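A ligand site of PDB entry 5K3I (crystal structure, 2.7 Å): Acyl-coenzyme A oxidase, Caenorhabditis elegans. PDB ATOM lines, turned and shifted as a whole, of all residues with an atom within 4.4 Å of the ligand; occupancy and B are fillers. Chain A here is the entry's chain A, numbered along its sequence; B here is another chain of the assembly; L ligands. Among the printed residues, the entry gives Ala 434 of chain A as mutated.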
ATOM      1  N   LEU A 115      17.560 -25.835 -23.350  1.00  0.00           N
ATOM      2  CA  LEU A 115      18.168 -25.351 -22.121  1.00  0.00           C
ATOM      3  C   LEU A 115      19.652 -25.658 -22.020  1.00  0.00           C
ATOM      4  O   LEU A 115      20.321 -25.130 -21.132  1.00  0.00           O
ATOM      5  CB  LEU A 115      17.435 -25.929 -20.914  1.00  0.00           C
ATOM      6  CG  LEU A 115      16.398 -24.867 -20.525  1.00  0.00           C
ATOM      7  CD1 LEU A 115      15.039 -25.194 -21.129  1.00  0.00           C
ATOM      8  CD2 LEU A 115      16.357 -24.709 -19.037  1.00  0.00           C
ATOM      9  N   TYR A 149      19.542 -26.967 -16.391  1.00  0.00           N
ATOM     10  CA  TYR A 149      19.737 -26.228 -15.148  1.00  0.00           C
ATOM     11  C   TYR A 149      18.531 -26.538 -14.268  1.00  0.00           C
ATOM     12  O   TYR A 149      17.399 -26.168 -14.612  1.00  0.00           O
ATOM     13  CB  TYR A 149      19.866 -24.724 -15.414  1.00  0.00           C
ATOM     14  CG  TYR A 149      20.147 -23.922 -14.176  1.00  0.00           C
ATOM     15  CD1 TYR A 149      21.429 -23.844 -13.658  1.00  0.00           C
ATOM     16  CD2 TYR A 149      19.124 -23.268 -13.508  1.00  0.00           C
ATOM     17  CE1 TYR A 149      21.696 -23.108 -12.522  1.00  0.00           C
ATOM     18  CE2 TYR A 149      19.369 -22.537 -12.371  1.00  0.00           C
ATOM     19  CZ  TYR A 149      20.647 -22.464 -11.884  1.00  0.00           C
ATOM     20  OH  TYR A 149      20.893 -21.734 -10.737  1.00  0.00           O
ATOM     21  N   ALA A 150      18.773 -27.227 -13.154  1.00  0.00           N
ATOM     22  CA  ALA A 150      17.707 -27.724 -12.290  1.00  0.00           C
ATOM     23  C   ALA A 150      17.660 -26.946 -10.978  1.00  0.00           C
ATOM     24  O   ALA A 150      18.341 -27.284 -10.015  1.00  0.00           O
ATOM     25  CB  ALA A 150      17.889 -29.221 -12.031  1.00  0.00           C
ATOM     26  N   GLN A 151      16.844 -25.897 -10.948  1.00  0.00           N
ATOM     27  CA  GLN A 151      16.642 -25.075  -9.751  1.00  0.00           C
ATOM     28  C   GLN A 151      15.294 -25.328  -9.087  1.00  0.00           C
ATOM     29  O   GLN A 151      15.237 -25.733  -7.921  1.00  0.00           O
ATOM     30  CB  GLN A 151      16.772 -23.604 -10.143  1.00  0.00           C
ATOM     31  CG  GLN A 151      16.663 -22.619  -9.007  1.00  0.00           C
ATOM     32  CD  GLN A 151      17.112 -21.236  -9.411  1.00  0.00           C
ATOM     33  OE1 GLN A 151      18.315 -20.971  -9.548  1.00  0.00           O
ATOM     34  NE2 GLN A 151      16.154 -20.344  -9.632  1.00  0.00           N
ATOM     35  N   THR A 152      14.202 -25.079  -9.817  1.00  0.00           N
ATOM     36  CA  THR A 152      12.856 -25.191  -9.273  1.00  0.00           C
ATOM     37  C   THR A 152      12.520 -26.602  -8.798  1.00  0.00           C
ATOM     38  O   THR A 152      12.945 -27.597  -9.396  1.00  0.00           O
ATOM     39  CB  THR A 152      11.845 -24.728 -10.319  1.00  0.00           C
ATOM     40  OG1 THR A 152      12.196 -23.401 -10.746  1.00  0.00           O
ATOM     41  CG2 THR A 152      10.414 -24.715  -9.780  1.00  0.00           C
ATOM     42  N   HIS A 156       8.764 -25.285  -4.484  1.00  0.00           N
ATOM     43  CA  HIS A 156       9.395 -23.974  -4.413  1.00  0.00           C
ATOM     44  C   HIS A 156      10.023 -23.622  -5.751  1.00  0.00           C
ATOM     45  O   HIS A 156      10.761 -24.426  -6.336  1.00  0.00           O
ATOM     46  CB  HIS A 156      10.473 -23.938  -3.332  1.00  0.00           C
ATOM     47  CG  HIS A 156       9.941 -24.082  -1.936  1.00  0.00           C
ATOM     48  ND1 HIS A 156       9.699 -25.313  -1.357  1.00  0.00           N
ATOM     49  CD2 HIS A 156       9.613 -23.158  -1.010  1.00  0.00           C
ATOM     50  CE1 HIS A 156       9.247 -25.131  -0.126  1.00  0.00           C
ATOM     51  NE2 HIS A 156       9.178 -23.837   0.104  1.00  0.00           N
ATOM     52  N   GLY A 157       9.723 -22.420  -6.213  1.00  0.00           N
ATOM     53  CA  GLY A 157      10.361 -21.827  -7.371  1.00  0.00           C
ATOM     54  C   GLY A 157      10.868 -20.437  -7.057  1.00  0.00           C
ATOM     55  O   GLY A 157      12.011 -20.089  -7.381  1.00  0.00           O
ATOM     56  N   THR A 158       9.988 -19.618  -6.482  1.00  0.00           N
ATOM     57  CA  THR A 158      10.351 -18.273  -6.046  1.00  0.00           C
ATOM     58  C   THR A 158      11.286 -18.284  -4.832  1.00  0.00           C
ATOM     59  O   THR A 158      12.305 -17.589  -4.820  1.00  0.00           O
ATOM     60  CB  THR A 158       9.079 -17.485  -5.737  1.00  0.00           C
ATOM     61  OG1 THR A 158       8.236 -17.494  -6.898  1.00  0.00           O
ATOM     62  CG2 THR A 158       9.397 -16.034  -5.383  1.00  0.00           C
ATOM     63  N   TRP A 189      10.153 -28.707 -13.360  1.00  0.00           N
ATOM     64  CA  TRP A 189      10.155 -27.688 -14.436  1.00  0.00           C
ATOM     65  C   TRP A 189      11.459 -27.491 -15.208  1.00  0.00           C
ATOM     66  O   TRP A 189      11.380 -26.908 -16.297  1.00  0.00           O
ATOM     67  CB  TRP A 189       9.684 -26.324 -13.939  1.00  0.00           C
ATOM     68  CG  TRP A 189       8.206 -26.245 -13.843  1.00  0.00           C
ATOM     69  CD1 TRP A 189       7.438 -26.230 -12.713  1.00  0.00           C
ATOM     70  CD2 TRP A 189       7.301 -26.237 -14.947  1.00  0.00           C
ATOM     71  NE1 TRP A 189       6.110 -26.176 -13.056  1.00  0.00           N
ATOM     72  CE2 TRP A 189       6.002 -26.181 -14.419  1.00  0.00           C
ATOM     73  CE3 TRP A 189       7.467 -26.252 -16.338  1.00  0.00           C
ATOM     74  CZ2 TRP A 189       4.880 -26.163 -15.225  1.00  0.00           C
ATOM     75  CZ3 TRP A 189       6.357 -26.228 -17.134  1.00  0.00           C
ATOM     76  CH2 TRP A 189       5.070 -26.180 -16.577  1.00  0.00           C
ATOM     77  N   PRO A 190      12.652 -27.875 -14.728  1.00  0.00           N
ATOM     78  CA  PRO A 190      13.835 -27.720 -15.581  1.00  0.00           C
ATOM     79  C   PRO A 190      13.597 -28.324 -16.961  1.00  0.00           C
ATOM     80  O   PRO A 190      13.220 -29.490 -17.105  1.00  0.00           O
ATOM     81  CB  PRO A 190      14.916 -28.484 -14.799  1.00  0.00           C
ATOM     82  CG  PRO A 190      14.526 -28.276 -13.416  1.00  0.00           C
ATOM     83  CD  PRO A 190      13.046 -28.393 -13.402  1.00  0.00           C
ATOM     84  N   GLY A 191      13.817 -27.503 -17.979  1.00  0.00           N
ATOM     85  CA  GLY A 191      13.539 -27.935 -19.330  1.00  0.00           C
ATOM     86  C   GLY A 191      14.542 -28.978 -19.795  1.00  0.00           C
ATOM     87  O   GLY A 191      15.708 -28.945 -19.420  1.00  0.00           O
ATOM     88  N   ASN A 250      10.107 -30.906 -20.207  1.00  0.00           N
ATOM     89  CA  ASN A 250      10.286 -30.420 -18.842  1.00  0.00           C
ATOM     90  C   ASN A 250      10.124 -31.590 -17.883  1.00  0.00           C
ATOM     91  O   ASN A 250       9.223 -32.425 -18.056  1.00  0.00           O
ATOM     92  CB  ASN A 250       9.275 -29.301 -18.537  1.00  0.00           C
ATOM     93  CG  ASN A 250       9.509 -28.052 -19.366  1.00  0.00           C
ATOM     94  OD1 ASN A 250       8.941 -27.891 -20.444  1.00  0.00           O
ATOM     95  ND2 ASN A 250      10.342 -27.156 -18.854  1.00  0.00           N
ATOM     96  N   GLY A 429       4.775 -17.756 -21.389  1.00  0.00           N
ATOM     97  CA  GLY A 429       5.452 -18.501 -20.338  1.00  0.00           C
ATOM     98  C   GLY A 429       6.495 -17.678 -19.607  1.00  0.00           C
ATOM     99  O   GLY A 429       6.775 -17.917 -18.434  1.00  0.00           O
ATOM    100  N   THR A 432       6.049 -16.129 -16.192  1.00  0.00           N
ATOM    101  CA  THR A 432       6.313 -16.900 -14.981  1.00  0.00           C
ATOM    102  C   THR A 432       7.754 -17.396 -14.867  1.00  0.00           C
ATOM    103  O   THR A 432       8.327 -17.319 -13.782  1.00  0.00           O
ATOM    104  CB  THR A 432       5.360 -18.077 -14.861  1.00  0.00           C
ATOM    105  OG1 THR A 432       5.349 -18.834 -16.076  1.00  0.00           O
ATOM    106  CG2 THR A 432       3.936 -17.584 -14.550  1.00  0.00           C
ATOM    107  N   TYR A 433       8.373 -17.904 -15.925  1.00  0.00           N
ATOM    108  CA  TYR A 433       9.748 -18.348 -15.769  1.00  0.00           C
ATOM    109  C   TYR A 433      10.688 -17.155 -15.622  1.00  0.00           C
ATOM    110  O   TYR A 433      10.359 -16.010 -15.929  1.00  0.00           O
ATOM    111  CB  TYR A 433      10.203 -19.261 -16.913  1.00  0.00           C
ATOM    112  CG  TYR A 433      10.336 -18.693 -18.331  1.00  0.00           C
ATOM    113  CD1 TYR A 433      11.348 -17.801 -18.662  1.00  0.00           C
ATOM    114  CD2 TYR A 433       9.523 -19.166 -19.355  1.00  0.00           C
ATOM    115  CE1 TYR A 433      11.492 -17.327 -19.954  1.00  0.00           C
ATOM    116  CE2 TYR A 433       9.665 -18.701 -20.648  1.00  0.00           C
ATOM    117  CZ  TYR A 433      10.646 -17.777 -20.941  1.00  0.00           C
ATOM    118  OH  TYR A 433      10.761 -17.335 -22.247  1.00  0.00           O
ATOM    119  N   ALA A 434      11.881 -17.458 -15.119  1.00  0.00           N
ATOM    120  CA  ALA A 434      12.921 -16.480 -14.809  1.00  0.00           C
ATOM    121  C   ALA A 434      12.461 -15.455 -13.779  1.00  0.00           C
ATOM    122  O   ALA A 434      12.943 -14.319 -13.757  1.00  0.00           O
ATOM    123  CB  ALA A 434      13.430 -15.777 -16.075  1.00  0.00           C
ATOM    124  N   GLY A 435      11.535 -15.843 -12.906  1.00  0.00           N
ATOM    125  CA  GLY A 435      11.025 -14.941 -11.882  1.00  0.00           C
ATOM    126  C   GLY A 435       9.570 -14.593 -12.100  1.00  0.00           C
ATOM    127  O   GLY A 435       9.252 -13.963 -13.108  1.00  0.00           O
ATOM    128  N   GLU A 436       8.669 -15.008 -11.223  1.00  0.00           N
ATOM    129  CA  GLU A 436       7.276 -14.580 -11.310  1.00  0.00           C
ATOM    130  C   GLU A 436       7.183 -13.059 -11.459  1.00  0.00           C
ATOM    131  O   GLU A 436       7.854 -12.318 -10.750  1.00  0.00           O
ATOM    132  CB  GLU A 436       6.489 -15.043 -10.082  1.00  0.00           C
ATOM    133  CG  GLU A 436       5.144 -15.682 -10.422  1.00  0.00           C
ATOM    134  CD  GLU A 436       4.185 -14.706 -11.085  1.00  0.00           C
ATOM    135  OE1 GLU A 436       3.593 -15.065 -12.123  1.00  0.00           O
ATOM    136  OE2 GLU A 436       4.042 -13.581 -10.564  1.00  0.00           O
ATOM    137  N   MET A 438       4.982 -10.767 -10.697  1.00  0.00           N
ATOM    138  CA  MET A 438       4.660 -10.021  -9.486  1.00  0.00           C
ATOM    139  C   MET A 438       5.871  -9.921  -8.574  1.00  0.00           C
ATOM    140  O   MET A 438       6.120  -8.874  -7.966  1.00  0.00           O
ATOM    141  CB  MET A 438       3.510 -10.698  -8.748  1.00  0.00           C
ATOM    142  CG  MET A 438       2.186 -10.695  -9.464  1.00  0.00           C
ATOM    143  SD  MET A 438       1.826  -9.056 -10.116  1.00  0.00           S
ATOM    144  CE  MET A 438       0.130  -8.894  -9.579  1.00  0.00           C
ATOM    145  N   VAL A 439       6.659 -10.999  -8.496  1.00  0.00           N
ATOM    146  CA  VAL A 439       7.800 -11.015  -7.599  1.00  0.00           C
ATOM    147  C   VAL A 439       8.920 -10.150  -8.143  1.00  0.00           C
ATOM    148  O   VAL A 439       9.616  -9.453  -7.392  1.00  0.00           O
ATOM    149  CB  VAL A 439       8.251 -12.463  -7.337  1.00  0.00           C
ATOM    150  CG1 VAL A 439       9.456 -12.489  -6.405  1.00  0.00           C
ATOM    151  CG2 VAL A 439       7.106 -13.272  -6.773  1.00  0.00           C
ATOM    152  N   LEU A 442       8.218  -6.486  -7.552  1.00  0.00           N
ATOM    153  CA  LEU A 442       8.519  -6.094  -6.179  1.00  0.00           C
ATOM    154  C   LEU A 442      10.019  -6.097  -5.898  1.00  0.00           C
ATOM    155  O   LEU A 442      10.485  -5.314  -5.060  1.00  0.00           O
ATOM    156  CB  LEU A 442       7.812  -7.011  -5.179  1.00  0.00           C
ATOM    157  CG  LEU A 442       6.283  -6.899  -5.156  1.00  0.00           C
ATOM    158  CD1 LEU A 442       5.716  -8.059  -4.366  1.00  0.00           C
ATOM    159  CD2 LEU A 442       5.914  -5.588  -4.532  1.00  0.00           C
ATOM    160  N   ARG B 320      -0.883 -23.620  -1.761  1.00  0.00           N
ATOM    161  CA  ARG B 320       0.480 -23.210  -2.097  1.00  0.00           C
ATOM    162  C   ARG B 320       1.040 -22.240  -1.051  1.00  0.00           C
ATOM    163  O   ARG B 320       0.540 -21.120  -0.906  1.00  0.00           O
ATOM    164  CB  ARG B 320       0.520 -22.572  -3.478  1.00  0.00           C
ATOM    165  CG  ARG B 320       1.897 -22.117  -4.001  1.00  0.00           C
ATOM    166  CD  ARG B 320       3.006 -23.179  -3.937  1.00  0.00           C
ATOM    167  NE  ARG B 320       4.133 -22.783  -4.780  1.00  0.00           N
ATOM    168  CZ  ARG B 320       4.971 -23.642  -5.369  1.00  0.00           C
ATOM    169  NH1 ARG B 320       4.822 -24.945  -5.162  1.00  0.00           N
ATOM    170  NH2 ARG B 320       5.960 -23.200  -6.145  1.00  0.00           N
ATOM    171  N   GLN B 322       4.592 -20.160   0.022  1.00  0.00           N
ATOM    172  CA  GLN B 322       5.772 -19.644  -0.662  1.00  0.00           C
ATOM    173  C   GLN B 322       6.237 -18.312  -0.091  1.00  0.00           C
ATOM    174  O   GLN B 322       5.570 -17.288  -0.286  1.00  0.00           O
ATOM    175  CB  GLN B 322       5.496 -19.472  -2.170  1.00  0.00           C
ATOM    176  CG  GLN B 322       6.719 -19.432  -3.085  1.00  0.00           C
ATOM    177  CD  GLN B 322       7.487 -20.754  -3.155  1.00  0.00           C
ATOM    178  OE1 GLN B 322       8.637 -20.775  -3.598  1.00  0.00           O
ATOM    179  NE2 GLN B 322       6.843 -21.854  -2.797  1.00  0.00           N
ATOM    180  N   VAL B 334       0.295 -18.309  -0.365  1.00  0.00           N
ATOM    181  CA  VAL B 334       0.396 -17.188  -1.308  1.00  0.00           C
ATOM    182  C   VAL B 334      -0.893 -16.380  -1.330  1.00  0.00           C
ATOM    183  O   VAL B 334      -0.869 -15.198  -1.702  1.00  0.00           O
ATOM    184  CB  VAL B 334       0.791 -17.674  -2.716  1.00  0.00           C
ATOM    185  CG1 VAL B 334       2.106 -18.419  -2.675  1.00  0.00           C
ATOM    186  CG2 VAL B 334      -0.300 -18.537  -3.308  1.00  0.00           C
ATOM    187  N   TYR B 337      -0.682 -12.653   0.152  1.00  0.00           N
ATOM    188  CA  TYR B 337      -0.044 -11.462  -0.394  1.00  0.00           C
ATOM    189  C   TYR B 337      -1.108 -10.586  -1.047  1.00  0.00           C
ATOM    190  O   TYR B 337      -1.952 -11.081  -1.798  1.00  0.00           O
ATOM    191  CB  TYR B 337       1.019 -11.845  -1.417  1.00  0.00           C
ATOM    192  CG  TYR B 337       2.171 -12.697  -0.867  1.00  0.00           C
ATOM    193  CD1 TYR B 337       3.075 -12.189   0.045  1.00  0.00           C
ATOM    194  CD2 TYR B 337       2.359 -14.022  -1.301  1.00  0.00           C
ATOM    195  CE1 TYR B 337       4.128 -12.955   0.534  1.00  0.00           C
ATOM    196  CE2 TYR B 337       3.409 -14.796  -0.824  1.00  0.00           C
ATOM    197  CZ  TYR B 337       4.288 -14.262   0.094  1.00  0.00           C
ATOM    198  OH  TYR B 337       5.332 -15.026   0.583  1.00  0.00           O
ATOM    199  N   THR B 339      -0.822  -8.684  -3.388  1.00  0.00           N
ATOM    200  CA  THR B 339      -0.618  -8.828  -4.821  1.00  0.00           C
ATOM    201  C   THR B 339      -1.379 -10.015  -5.383  1.00  0.00           C
ATOM    202  O   THR B 339      -1.864  -9.960  -6.523  1.00  0.00           O
ATOM    203  CB  THR B 339       0.901  -8.937  -5.066  1.00  0.00           C
ATOM    204  OG1 THR B 339       1.395  -7.723  -5.672  1.00  0.00           O
ATOM    205  CG2 THR B 339       1.264 -10.141  -5.916  1.00  0.00           C
ATOM    206  N   GLN B 340      -1.525 -11.091  -4.602  1.00  0.00           N
ATOM    207  CA  GLN B 340      -2.255 -12.282  -5.045  1.00  0.00           C
ATOM    208  C   GLN B 340      -3.762 -12.076  -4.917  1.00  0.00           C
ATOM    209  O   GLN B 340      -4.520 -12.389  -5.847  1.00  0.00           O
ATOM    210  CB  GLN B 340      -1.815 -13.506  -4.239  1.00  0.00           C
ATOM    211  CG  GLN B 340      -2.461 -14.839  -4.638  1.00  0.00           C
ATOM    212  CD  GLN B 340      -1.694 -15.534  -5.735  1.00  0.00           C
ATOM    213  OE1 GLN B 340      -0.809 -14.946  -6.340  1.00  0.00           O
ATOM    214  NE2 GLN B 340      -2.011 -16.803  -5.979  1.00  0.00           N
ATOM    215  N   ARG B 343      -4.867  -9.903  -7.704  1.00  0.00           N
ATOM    216  CA  ARG B 343      -4.918 -10.519  -9.036  1.00  0.00           C
ATOM    217  C   ARG B 343      -5.996 -11.594  -9.187  1.00  0.00           C
ATOM    218  O   ARG B 343      -6.177 -12.107 -10.293  1.00  0.00           O
ATOM    219  CB  ARG B 343      -3.539 -11.082  -9.426  1.00  0.00           C
ATOM    220  CG  ARG B 343      -3.233 -12.532  -9.055  1.00  0.00           C
ATOM    221  CD  ARG B 343      -1.754 -12.831  -9.358  1.00  0.00           C
ATOM    222  NE  ARG B 343      -1.381 -12.453 -10.729  1.00  0.00           N
ATOM    223  CZ  ARG B 343      -0.249 -12.801 -11.324  1.00  0.00           C
ATOM    224  NH1 ARG B 343       0.649 -13.541 -10.681  1.00  0.00           N
ATOM    225  NH2 ARG B 343       0.006 -12.403 -12.563  1.00  0.00           N
ATOM    226  N   MET B 407      -1.610 -17.546 -14.090  1.00  0.00           N
ATOM    227  CA  MET B 407      -0.269 -17.135 -13.675  1.00  0.00           C
ATOM    228  C   MET B 407      -0.160 -17.048 -12.166  1.00  0.00           C
ATOM    229  O   MET B 407       0.951 -17.097 -11.628  1.00  0.00           O
ATOM    230  CB  MET B 407       0.110 -15.787 -14.293  1.00  0.00           C
ATOM    231  CG  MET B 407       0.275 -15.807 -15.796  1.00  0.00           C
ATOM    232  SD  MET B 407       0.734 -14.194 -16.438  1.00  0.00           S
ATOM    233  CE  MET B 407      -0.815 -13.304 -16.362  1.00  0.00           C
ATOM    234  N   ALA B 408      -1.297 -16.942 -11.467  1.00  0.00           N
ATOM    235  CA  ALA B 408      -1.335 -16.978 -10.010  1.00  0.00           C
ATOM    236  C   ALA B 408      -1.024 -18.353  -9.445  1.00  0.00           C
ATOM    237  O   ALA B 408      -0.817 -18.475  -8.239  1.00  0.00           O
ATOM    238  CB  ALA B 408      -2.711 -16.534  -9.517  1.00  0.00           C
ATOM    239  N   CYS B 409      -1.003 -19.393 -10.270  1.00  0.00           N
ATOM    240  CA  CYS B 409      -0.539 -20.709  -9.867  1.00  0.00           C
ATOM    241  C   CYS B 409       0.948 -20.917 -10.095  1.00  0.00           C
ATOM    242  O   CYS B 409       1.430 -22.033  -9.883  1.00  0.00           O
ATOM    243  CB  CYS B 409      -1.316 -21.803 -10.615  1.00  0.00           C
ATOM    244  SG  CYS B 409      -3.085 -21.761 -10.347  1.00  0.00           S
ATOM    245  N   GLY B 410       1.695 -19.885 -10.520  1.00  0.00           N
ATOM    246  CA  GLY B 410       3.118 -20.089 -10.663  1.00  0.00           C
ATOM    247  C   GLY B 410       3.355 -21.052 -11.813  1.00  0.00           C
ATOM    248  O   GLY B 410       2.522 -21.218 -12.695  1.00  0.00           O
ATOM    249  N   GLY B 411       4.545 -21.659 -11.794  1.00  0.00           N
ATOM    250  CA  GLY B 411       4.965 -22.590 -12.827  1.00  0.00           C
ATOM    251  C   GLY B 411       3.874 -23.590 -13.188  1.00  0.00           C
ATOM    252  O   GLY B 411       3.560 -23.759 -14.364  1.00  0.00           O
ATOM    253  N   TYR B 414       1.136 -23.323 -15.913  1.00  0.00           N
ATOM    254  CA  TYR B 414       1.468 -23.556 -17.307  1.00  0.00           C
ATOM    255  C   TYR B 414       1.279 -25.014 -17.690  1.00  0.00           C
ATOM    256  O   TYR B 414       1.192 -25.307 -18.888  1.00  0.00           O
ATOM    257  CB  TYR B 414       2.907 -23.114 -17.561  1.00  0.00           C
ATOM    258  CG  TYR B 414       3.259 -22.887 -19.005  1.00  0.00           C
ATOM    259  CD1 TYR B 414       2.866 -21.737 -19.672  1.00  0.00           C
ATOM    260  CD2 TYR B 414       3.994 -23.828 -19.713  1.00  0.00           C
ATOM    261  CE1 TYR B 414       3.182 -21.529 -20.996  1.00  0.00           C
ATOM    262  CE2 TYR B 414       4.321 -23.623 -21.037  1.00  0.00           C
ATOM    263  CZ  TYR B 414       3.910 -22.473 -21.673  1.00  0.00           C
ATOM    264  OH  TYR B 414       4.220 -22.253 -22.995  1.00  0.00           O
HETATM  265  P1  LIG L   1       4.784 -19.450  -6.994  1.00  0.00           P
HETATM  266  O1  LIG L   1       5.679 -18.538  -6.190  1.00  0.00           O
HETATM  267  O2  LIG L   1       4.635 -20.776  -6.274  1.00  0.00           O
HETATM  268  O3  LIG L   1       3.333 -18.704  -7.170  1.00  0.00           O
HETATM  269  C1  LIG L   1       3.463 -17.379  -7.636  1.00  0.00           C
HETATM  270  C2  LIG L   1       2.196 -16.654  -7.115  1.00  0.00           C
HETATM  271  O4  LIG L   1       2.316 -16.420  -5.847  1.00  0.00           O
HETATM  272  C3  LIG L   1       2.215 -15.331  -7.879  1.00  0.00           C
HETATM  273  O5  LIG L   1       0.942 -14.963  -8.185  1.00  0.00           O
HETATM  274  C4  LIG L   1       2.888 -14.324  -6.926  1.00  0.00           C
HETATM  275  O6  LIG L   1       2.020 -13.106  -6.896  1.00  0.00           O
HETATM  276  C5  LIG L   1       2.827 -14.886  -5.744  1.00  0.00           C
HETATM  277  N1  LIG L   1       4.035 -14.842  -4.943  1.00  0.00           N
HETATM  278  C6  LIG L   1       4.942 -15.813  -4.732  1.00  0.00           C
HETATM  279  N2  LIG L   1       5.871 -15.338  -3.918  1.00  0.00           N
HETATM  280  C7  LIG L   1       5.530 -14.053  -3.593  1.00  0.00           C
HETATM  281  C8  LIG L   1       6.097 -13.079  -2.811  1.00  0.00           C
HETATM  282  N3  LIG L   1       7.262 -12.924  -1.980  1.00  0.00           N
HETATM  283  N4  LIG L   1       5.510 -11.881  -2.690  1.00  0.00           N
HETATM  284  C9  LIG L   1       4.346 -11.615  -3.342  1.00  0.00           C
HETATM  285  N5  LIG L   1       3.797 -12.564  -4.111  1.00  0.00           N
HETATM  286  C10 LIG L   1       4.381 -13.771  -4.234  1.00  0.00           C
HETATM  287  N6  LIG L   1      12.610 -23.713 -13.385  1.00  0.00           N
HETATM  288  C11 LIG L   1      13.999 -24.194 -13.428  1.00  0.00           C
HETATM  289  O7  LIG L   1      14.616 -24.309 -12.385  1.00  0.00           O
HETATM  290  N7  LIG L   1      14.586 -24.510 -14.748  1.00  0.00           N
HETATM  291  C12 LIG L   1      13.790 -24.348 -15.955  1.00  0.00           C
HETATM  292  O8  LIG L   1      14.233 -24.596 -17.003  1.00  0.00           O
HETATM  293  C13 LIG L   1      12.372 -23.861 -15.900  1.00  0.00           C
HETATM  294  N8  LIG L   1      11.560 -23.688 -17.084  1.00  0.00           N
HETATM  295  C14 LIG L   1      10.170 -23.196 -16.968  1.00  0.00           C
HETATM  296  C15 LIG L   1       9.414 -23.049 -18.140  1.00  0.00           C
HETATM  297  C16 LIG L   1       8.090 -22.583 -18.032  1.00  0.00           C
HETATM  298  C17 LIG L   1       7.537 -22.519 -19.471  1.00  0.00           C
HETATM  299  C18 LIG L   1       7.526 -22.273 -16.775  1.00  0.00           C
HETATM  300  C19 LIG L   1       6.093 -21.779 -16.676  1.00  0.00           C
HETATM  301  C20 LIG L   1       8.298 -22.434 -15.606  1.00  0.00           C
HETATM  302  C21 LIG L   1       9.623 -22.899 -15.724  1.00  0.00           C
HETATM  303  N9  LIG L   1      10.469 -23.078 -14.492  1.00  0.00           N
HETATM  304  C22 LIG L   1      11.822 -23.549 -14.612  1.00  0.00           C
HETATM  305  C23 LIG L   1       9.933 -22.763 -13.175  1.00  0.00           C
HETATM  306  C24 LIG L   1       9.980 -21.240 -12.925  1.00  0.00           C
HETATM  307  O9  LIG L   1      11.272 -20.809 -12.635  1.00  0.00           O
HETATM  308  C25 LIG L   1       9.054 -20.997 -11.739  1.00  0.00           C
HETATM  309  O10 LIG L   1       7.838 -21.562 -12.095  1.00  0.00           O
HETATM  310  C26 LIG L   1       8.947 -19.488 -11.565  1.00  0.00           C
HETATM  311  O11 LIG L   1      10.081 -19.042 -10.899  1.00  0.00           O
HETATM  312  C27 LIG L   1       7.726 -19.134 -10.720  1.00  0.00           C
HETATM  313  O12 LIG L   1       7.977 -19.485  -9.370  1.00  0.00           O
HETATM  314  P2  LIG L   1       6.836 -20.485  -8.714  1.00  0.00           P
HETATM  315  O13 LIG L   1       6.544 -21.625  -9.680  1.00  0.00           O
HETATM  316  O14 LIG L   1       7.268 -21.062  -7.400  1.00  0.00           O
HETATM  317  O15 LIG L   1       5.420 -19.658  -8.503  1.00  0.00           O
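O8 of the ligand lies within hydrogen-bond range of N of Gly 191 (3.1 Å).
An oxygen (O14) of the ligand sits at hydrogen-bond distance from the backbone NH (N) of Thr 158, 3.2 Å away.
N of Gln 151 sits at hydrogen-bond distance from O7 of the ligand (3.1 Å).
An oxygen (O1) of the ligand lies within hydrogen-bond range of the side-chain hydroxyl of Thr 158 (2.9 Å).
The backbone NH (N) of Gly 411 of chain B is in hydrogen-bond range of an oxygen (O13) of the ligand (2.9 Å).
A nitrogen (N7) of the ligand is in hydrogen-bond range of the backbone carbonyl oxygen of Tyr 149 (3.3 Å).
The backbone NH (N) of Thr 152 lies within hydrogen-bond range of an oxygen (O7) of the ligand, 2.7 Å away.
N of Gly 157 lies within hydrogen-bond range of O14 of the ligand (3.0 Å).
The guanidinium group (NE) of Arg 320 of chain B is in salt-bridge range of an oxygen (O2) of the ligand.
The side-chain amide oxygen of Gln 340 of chain B is in hydrogen-bond range of an oxygen (O5) of the ligand, at 2.5 Å.
NH1 of Arg 343 of chain B lies within hydrogen-bond range of O5 of the ligand (2.9 Å).
The side-chain hydroxyl (OG1) of Thr 152 lies within hydrogen-bond range of a nitrogen (N6) of the ligand, 2.7 Å away.
O of Gln 322 of chain B lies within hydrogen-bond range of OH of Tyr 337 of chain B, at 2.4 Å.
OH of Tyr 149 is in hydrogen-bond range of OE1 of Gln 151, 2.9 Å away.
The side-chain amide nitrogen (NE2) of Gln 340 of chain B lies within hydrogen-bond range of the backbone carbonyl oxygen (O) of Ala 408 of chain B (3.1 Å).
NE2 of Gln 322 of chain B sits close to NE of Arg 320 of chain B, 3.5 Å away.
The guanidinium group (NH1) of Arg 343 of chain B is in salt-bridge range of the side-chain carboxylate (OE2) of Glu 436, at 3.4 Å.
O of Trp 189 lies within hydrogen-bond range of ND2 of Asn 250, 2.8 Å away.
N of Thr 158 is in hydrogen-bond range of OE1 of Gln 322 of chain B (3.4 Å).
N of Met 438 lies within hydrogen-bond range of OE2 of Glu 436 (3.0 Å).
N8 of the ligand lies close to O of Trp 189, at 3.3 Å.
Leu 115 touches the ligand (CD2 to O8, 2.9 Å).
CA of Pro 190 touches C12 of the ligand, at 3.4 Å.
OG1 of Thr 432 touches C19 of the ligand (3.1 Å).
Tyr 433 touches the ligand.
Glu 436 touches the ligand (CG to C1, 3.7 Å).
CB of Met 438 touches O6 of the ligand, at 3.4 Å.
CG2 of Val 439 touches C7 of the ligand, 3.6 Å away.
Leu 442 touches the ligand.
Gln 322 of chain B touches the ligand.
Val 334 of chain B touches the ligand.
CG of Tyr 337 of chain B touches C9 of the ligand, 3.5 Å away.
Thr 339 of chain B touches the ligand (CG2 to O6, 3.2 Å).
Ala 408 of chain B touches the ligand.
Gly 410 of chain B touches the ligand (CA to O15, 3.2 Å).
Tyr 414 of chain B touches the ligand (CB to C19, 3.6 Å).
Hydrophobic or aromatic side chains within 4 Å of the ligand: Leu 115, Trp 189, Pro 190, Tyr 433, Met 438, Val 439, Leu 442, Val 334 of chain B, Tyr 337 of chain B and Tyr 414 of chain B.
Within 4 Å of the ligand: Leu 115, Tyr 149, Gln 151, Thr 152, Gly 157, Thr 158, Trp 189, Pro 190, Gly 191, Thr 432, Tyr 433, Glu 436, Met 438, Val 439, Leu 442, Arg 320 of chain B, Gln 322 of chain B, Val 334 of chain B, Tyr 337 of chain B, Thr 339 of chain B, Gln 340 of chain B, Arg 343 of chain B, Ala 408 of chain B, Gly 410 of chain B, Gly 411 of chain B and Tyr 414 of chain B.
Along chain A the residues within 4 Å of the ligand span positions 115 to 442.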
